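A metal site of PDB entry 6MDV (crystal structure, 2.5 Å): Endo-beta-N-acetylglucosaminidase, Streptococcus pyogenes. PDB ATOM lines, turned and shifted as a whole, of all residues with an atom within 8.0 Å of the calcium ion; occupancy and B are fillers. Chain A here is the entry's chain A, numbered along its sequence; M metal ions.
CA of Ile 658 touches the calcium ion (3.9 Å). Of the 20 residues printed, 7 come within 4 Å of the calcium ion. The nearest printed residue that does not touch the calcium ion is Lys 663 (4.4 Å).
The backbone carbonyl oxygen (O) of Phe 692 is in hydrogen-bond range of the backbone NH (N) of Thr 782 (2.9 Å). OG1 of Thr 696 is in hydrogen-bond range of OG1 of Thr 782, at 2.8 Å. The backbone NH of Phe 692 is in hydrogen-bond range of the backbone carbonyl oxygen of Glu 783. The backbone NH of Leu 784 is in hydrogen-bond range of the backbone carbonyl oxygen of Ile 658 (2.9 Å).
The calcium ion is bound by O of Lys 657 (2.3 Å), O of Glu 662 (2.5 Å), OD1 of Asp 660 (2.5 Å), O of Thr 782 (2.6 Å), OE1 of Glu 783 (2.7 Å), OD2 of Asp 665 (2.8 Å) and OD1 of Asp 665 (2.8 Å).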
ATOM      1  N   GLN A 654      -4.585 -11.982   9.912  1.00  0.00           N
ATOM      2  CA  GLN A 654      -3.681 -13.066   9.538  1.00  0.00           C
ATOM      3  C   GLN A 654      -3.466 -14.034  10.687  1.00  0.00           C
ATOM      4  O   GLN A 654      -3.235 -15.222  10.451  1.00  0.00           O
ATOM      5  CB  GLN A 654      -2.352 -12.536   9.018  1.00  0.00           C
ATOM      6  CG  GLN A 654      -2.534 -11.524   7.941  1.00  0.00           C
ATOM      7  CD  GLN A 654      -2.704 -12.194   6.589  1.00  0.00           C
ATOM      8  OE1 GLN A 654      -2.381 -13.385   6.436  1.00  0.00           O
ATOM      9  NE2 GLN A 654      -3.272 -11.464   5.624  1.00  0.00           N
ATOM     10  N   ALA A 655      -3.573 -13.548  11.928  1.00  0.00           N
ATOM     11  CA  ALA A 655      -3.474 -14.449  13.071  1.00  0.00           C
ATOM     12  C   ALA A 655      -4.580 -15.471  13.035  1.00  0.00           C
ATOM     13  O   ALA A 655      -4.390 -16.618  13.455  1.00  0.00           O
ATOM     14  CB  ALA A 655      -3.538 -13.647  14.375  1.00  0.00           C
ATOM     15  N   LYS A 656      -5.737 -15.080  12.508  1.00  0.00           N
ATOM     16  CA  LYS A 656      -6.872 -15.989  12.544  1.00  0.00           C
ATOM     17  C   LYS A 656      -6.647 -17.203  11.657  1.00  0.00           C
ATOM     18  O   LYS A 656      -7.272 -18.252  11.868  1.00  0.00           O
ATOM     19  CB  LYS A 656      -8.145 -15.262  12.132  1.00  0.00           C
ATOM     20  CG  LYS A 656      -8.656 -14.298  13.176  1.00  0.00           C
ATOM     21  CD  LYS A 656      -9.686 -13.318  12.593  1.00  0.00           C
ATOM     22  CE  LYS A 656     -10.534 -12.610  13.717  1.00  0.00           C
ATOM     23  NZ  LYS A 656     -11.646 -11.792  13.093  1.00  0.00           N
ATOM     24  N   LYS A 657      -5.763 -17.097  10.693  1.00  0.00           N
ATOM     25  CA  LYS A 657      -5.656 -18.167   9.713  1.00  0.00           C
ATOM     26  C   LYS A 657      -4.809 -19.335  10.182  1.00  0.00           C
ATOM     27  O   LYS A 657      -4.692 -20.323   9.454  1.00  0.00           O
ATOM     28  CB  LYS A 657      -5.091 -17.577   8.423  1.00  0.00           C
ATOM     29  CG  LYS A 657      -6.012 -16.543   7.782  1.00  0.00           C
ATOM     30  CD  LYS A 657      -5.352 -15.888   6.579  1.00  0.00           C
ATOM     31  CE  LYS A 657      -6.321 -14.968   5.854  1.00  0.00           C
ATOM     32  NZ  LYS A 657      -5.621 -14.206   4.791  1.00  0.00           N
ATOM     33  N   ILE A 658      -4.228 -19.302  11.385  1.00  0.00           N
ATOM     34  CA  ILE A 658      -3.424 -20.432  11.818  1.00  0.00           C
ATOM     35  C   ILE A 658      -4.326 -21.435  12.534  1.00  0.00           C
ATOM     36  O   ILE A 658      -3.840 -22.396  13.144  1.00  0.00           O
ATOM     37  CB  ILE A 658      -2.259 -20.021  12.719  1.00  0.00           C
ATOM     38  CG1 ILE A 658      -2.798 -19.512  14.035  1.00  0.00           C
ATOM     39  CG2 ILE A 658      -1.396 -18.988  12.045  1.00  0.00           C
ATOM     40  CD1 ILE A 658      -1.728 -19.443  15.093  1.00  0.00           C
ATOM     41  N   PHE A 659      -5.633 -21.207  12.486  1.00  0.00           N
ATOM     42  CA  PHE A 659      -6.611 -22.070  13.122  1.00  0.00           C
ATOM     43  C   PHE A 659      -7.711 -22.495  12.159  1.00  0.00           C
ATOM     44  O   PHE A 659      -8.692 -23.100  12.590  1.00  0.00           O
ATOM     45  CB  PHE A 659      -7.247 -21.385  14.328  1.00  0.00           C
ATOM     46  CG  PHE A 659      -6.265 -20.994  15.390  1.00  0.00           C
ATOM     47  CD1 PHE A 659      -5.461 -21.953  15.983  1.00  0.00           C
ATOM     48  CD2 PHE A 659      -6.117 -19.670  15.761  1.00  0.00           C
ATOM     49  CE1 PHE A 659      -4.553 -21.599  16.968  1.00  0.00           C
ATOM     50  CE2 PHE A 659      -5.207 -19.307  16.740  1.00  0.00           C
ATOM     51  CZ  PHE A 659      -4.424 -20.268  17.341  1.00  0.00           C
ATOM     52  N   ASP A 660      -7.588 -22.162  10.871  1.00  0.00           N
ATOM     53  CA  ASP A 660      -8.454 -22.758   9.869  1.00  0.00           C
ATOM     54  C   ASP A 660      -7.970 -24.188   9.611  1.00  0.00           C
ATOM     55  O   ASP A 660      -7.153 -24.728  10.359  1.00  0.00           O
ATOM     56  CB  ASP A 660      -8.522 -21.887   8.612  1.00  0.00           C
ATOM     57  CG  ASP A 660      -7.150 -21.656   7.965  1.00  0.00           C
ATOM     58  OD1 ASP A 660      -6.262 -22.518   8.071  1.00  0.00           O
ATOM     59  OD2 ASP A 660      -6.989 -20.598   7.317  1.00  0.00           O
ATOM     60  N   GLY A 661      -8.474 -24.837   8.589  1.00  0.00           N
ATOM     61  CA  GLY A 661      -7.979 -26.191   8.488  1.00  0.00           C
ATOM     62  C   GLY A 661      -6.769 -26.356   7.610  1.00  0.00           C
ATOM     63  O   GLY A 661      -6.280 -27.472   7.465  1.00  0.00           O
ATOM     64  N   GLU A 662      -6.292 -25.263   7.009  1.00  0.00           N
ATOM     65  CA  GLU A 662      -5.440 -25.337   5.826  1.00  0.00           C
ATOM     66  C   GLU A 662      -4.016 -24.854   6.151  1.00  0.00           C
ATOM     67  O   GLU A 662      -3.735 -24.273   7.203  1.00  0.00           O
ATOM     68  CB  GLU A 662      -6.040 -24.525   4.668  1.00  0.00           C
ATOM     69  CG  GLU A 662      -7.566 -24.475   4.659  1.00  0.00           C
ATOM     70  CD  GLU A 662      -8.174 -25.711   4.045  1.00  0.00           C
ATOM     71  OE1 GLU A 662      -7.483 -26.462   3.335  1.00  0.00           O
ATOM     72  OE2 GLU A 662      -9.372 -25.944   4.277  1.00  0.00           O
ATOM     73  N   LYS A 663      -3.117 -25.132   5.211  1.00  0.00           N
ATOM     74  CA  LYS A 663      -1.728 -24.674   5.265  1.00  0.00           C
ATOM     75  C   LYS A 663      -1.448 -23.674   4.158  1.00  0.00           C
ATOM     76  O   LYS A 663      -0.300 -23.478   3.756  1.00  0.00           O
ATOM     77  CB  LYS A 663      -0.786 -25.885   5.198  1.00  0.00           C
ATOM     78  CG  LYS A 663      -0.813 -26.843   6.457  1.00  0.00           C
ATOM     79  CD  LYS A 663      -2.141 -27.614   6.638  1.00  0.00           C
ATOM     80  CE  LYS A 663      -2.114 -28.636   7.798  1.00  0.00           C
ATOM     81  NZ  LYS A 663      -3.484 -29.239   8.155  1.00  0.00           N
ATOM     82  N   SER A 664      -2.501 -23.048   3.641  1.00  0.00           N
ATOM     83  CA  SER A 664      -2.488 -22.155   2.479  1.00  0.00           C
ATOM     84  C   SER A 664      -2.481 -20.703   2.899  1.00  0.00           C
ATOM     85  O   SER A 664      -3.287 -19.902   2.435  1.00  0.00           O
ATOM     86  CB  SER A 664      -3.699 -22.432   1.603  1.00  0.00           C
ATOM     87  OG  SER A 664      -4.876 -22.102   2.338  1.00  0.00           O
ATOM     88  N   ASP A 665      -1.555 -20.330   3.779  1.00  0.00           N
ATOM     89  CA  ASP A 665      -1.525 -19.011   4.390  1.00  0.00           C
ATOM     90  C   ASP A 665      -0.268 -18.959   5.238  1.00  0.00           C
ATOM     91  O   ASP A 665       0.400 -19.966   5.460  1.00  0.00           O
ATOM     92  CB  ASP A 665      -2.762 -18.763   5.248  1.00  0.00           C
ATOM     93  CG  ASP A 665      -3.034 -19.918   6.220  1.00  0.00           C
ATOM     94  OD1 ASP A 665      -2.232 -20.128   7.164  1.00  0.00           O
ATOM     95  OD2 ASP A 665      -4.055 -20.627   6.037  1.00  0.00           O
ATOM     96  N   ARG A 666       0.064 -17.769   5.687  1.00  0.00           N
ATOM     97  CA  ARG A 666       1.223 -17.639   6.552  1.00  0.00           C
ATOM     98  C   ARG A 666       0.928 -16.531   7.544  1.00  0.00           C
ATOM     99  O   ARG A 666       0.156 -15.621   7.257  1.00  0.00           O
ATOM    100  CB  ARG A 666       2.484 -17.375   5.735  1.00  0.00           C
ATOM    101  CG  ARG A 666       2.331 -16.178   4.848  1.00  0.00           C
ATOM    102  CD  ARG A 666       3.464 -16.022   3.857  1.00  0.00           C
ATOM    103  NE  ARG A 666       3.251 -14.811   3.068  1.00  0.00           N
ATOM    104  CZ  ARG A 666       3.901 -14.510   1.953  1.00  0.00           C
ATOM    105  NH1 ARG A 666       4.837 -15.319   1.462  1.00  0.00           N
ATOM    106  NH2 ARG A 666       3.615 -13.370   1.333  1.00  0.00           N
ATOM    107  N   PHE A 667       1.495 -16.658   8.733  1.00  0.00           N
ATOM    108  CA  PHE A 667       1.489 -15.605   9.728  1.00  0.00           C
ATOM    109  C   PHE A 667       2.922 -15.250  10.072  1.00  0.00           C
ATOM    110  O   PHE A 667       3.700 -16.117  10.489  1.00  0.00           O
ATOM    111  CB  PHE A 667       0.737 -15.991  10.983  1.00  0.00           C
ATOM    112  CG  PHE A 667       0.924 -15.028  12.100  1.00  0.00           C
ATOM    113  CD1 PHE A 667       0.123 -13.912  12.196  1.00  0.00           C
ATOM    114  CD2 PHE A 667       1.915 -15.215  13.042  1.00  0.00           C
ATOM    115  CE1 PHE A 667       0.302 -13.006  13.216  1.00  0.00           C
ATOM    116  CE2 PHE A 667       2.099 -14.326  14.059  1.00  0.00           C
ATOM    117  CZ  PHE A 667       1.285 -13.212  14.148  1.00  0.00           C
ATOM    118  N   PHE A 692       2.717 -26.294  12.106  1.00  0.00           N
ATOM    119  CA  PHE A 692       3.077 -26.503  10.713  1.00  0.00           C
ATOM    120  C   PHE A 692       3.926 -25.327  10.259  1.00  0.00           C
ATOM    121  O   PHE A 692       3.453 -24.180  10.229  1.00  0.00           O
ATOM    122  CB  PHE A 692       1.817 -26.683   9.863  1.00  0.00           C
ATOM    123  CG  PHE A 692       1.102 -27.975  10.126  1.00  0.00           C
ATOM    124  CD1 PHE A 692       1.450 -29.127   9.419  1.00  0.00           C
ATOM    125  CD2 PHE A 692       0.112 -28.048  11.078  1.00  0.00           C
ATOM    126  CE1 PHE A 692       0.807 -30.328   9.661  1.00  0.00           C
ATOM    127  CE2 PHE A 692      -0.552 -29.249  11.327  1.00  0.00           C
ATOM    128  CZ  PHE A 692      -0.201 -30.394  10.614  1.00  0.00           C
ATOM    129  N   THR A 696       5.546 -25.624   5.031  1.00  0.00           N
ATOM    130  CA  THR A 696       4.324 -26.345   4.687  1.00  0.00           C
ATOM    131  C   THR A 696       3.368 -25.508   3.839  1.00  0.00           C
ATOM    132  O   THR A 696       2.281 -25.997   3.496  1.00  0.00           O
ATOM    133  CB  THR A 696       3.553 -26.786   5.946  1.00  0.00           C
ATOM    134  OG1 THR A 696       2.923 -25.652   6.558  1.00  0.00           O
ATOM    135  CG2 THR A 696       4.472 -27.469   6.953  1.00  0.00           C
ATOM    136  N   TYR A 781       4.779 -19.316  10.023  1.00  0.00           N
ATOM    137  CA  TYR A 781       4.154 -20.623  10.180  1.00  0.00           C
ATOM    138  C   TYR A 781       2.723 -20.528   9.652  1.00  0.00           C
ATOM    139  O   TYR A 781       2.180 -19.435   9.419  1.00  0.00           O
ATOM    140  CB  TYR A 781       4.228 -21.133  11.632  1.00  0.00           C
ATOM    141  CG  TYR A 781       3.517 -20.316  12.678  1.00  0.00           C
ATOM    142  CD1 TYR A 781       4.065 -19.134  13.198  1.00  0.00           C
ATOM    143  CD2 TYR A 781       2.315 -20.759  13.209  1.00  0.00           C
ATOM    144  CE1 TYR A 781       3.403 -18.400  14.169  1.00  0.00           C
ATOM    145  CE2 TYR A 781       1.656 -20.049  14.184  1.00  0.00           C
ATOM    146  CZ  TYR A 781       2.201 -18.867  14.668  1.00  0.00           C
ATOM    147  OH  TYR A 781       1.503 -18.171  15.627  1.00  0.00           O
ATOM    148  N   THR A 782       2.121 -21.690   9.396  1.00  0.00           N
ATOM    149  CA  THR A 782       0.848 -21.738   8.700  1.00  0.00           C
ATOM    150  C   THR A 782      -0.306 -22.222   9.553  1.00  0.00           C
ATOM    151  O   THR A 782      -1.447 -21.803   9.325  1.00  0.00           O
ATOM    152  CB  THR A 782       0.966 -22.647   7.461  1.00  0.00           C
ATOM    153  OG1 THR A 782       1.035 -24.017   7.881  1.00  0.00           O
ATOM    154  CG2 THR A 782       2.230 -22.322   6.676  1.00  0.00           C
ATOM    155  N   GLU A 783      -0.053 -23.071  10.550  1.00  0.00           N
ATOM    156  CA  GLU A 783      -1.141 -23.722  11.256  1.00  0.00           C
ATOM    157  C   GLU A 783      -0.633 -24.182  12.610  1.00  0.00           C
ATOM    158  O   GLU A 783       0.503 -24.640  12.716  1.00  0.00           O
ATOM    159  CB  GLU A 783      -1.685 -24.901  10.435  1.00  0.00           C
ATOM    160  CG  GLU A 783      -2.810 -25.673  11.084  1.00  0.00           C
ATOM    161  CD  GLU A 783      -4.136 -24.946  11.011  1.00  0.00           C
ATOM    162  OE1 GLU A 783      -4.261 -23.993  10.202  1.00  0.00           O
ATOM    163  OE2 GLU A 783      -5.064 -25.334  11.753  1.00  0.00           O
ATOM    164  N   LEU A 784      -1.486 -24.065  13.627  1.00  0.00           N
ATOM    165  CA  LEU A 784      -1.169 -24.465  14.990  1.00  0.00           C
ATOM    166  C   LEU A 784      -2.254 -25.419  15.498  1.00  0.00           C
ATOM    167  O   LEU A 784      -3.439 -25.166  15.307  1.00  0.00           O
ATOM    168  CB  LEU A 784      -1.052 -23.252  15.903  1.00  0.00           C
ATOM    169  CG  LEU A 784      -0.441 -23.488  17.286  1.00  0.00           C
ATOM    170  CD1 LEU A 784       0.917 -24.105  17.177  1.00  0.00           C
ATOM    171  CD2 LEU A 784      -0.356 -22.161  17.998  1.00  0.00           C
HETATM  172 CA    CA M   1      -3.833 -22.100   8.360  1.00  0.00          CA
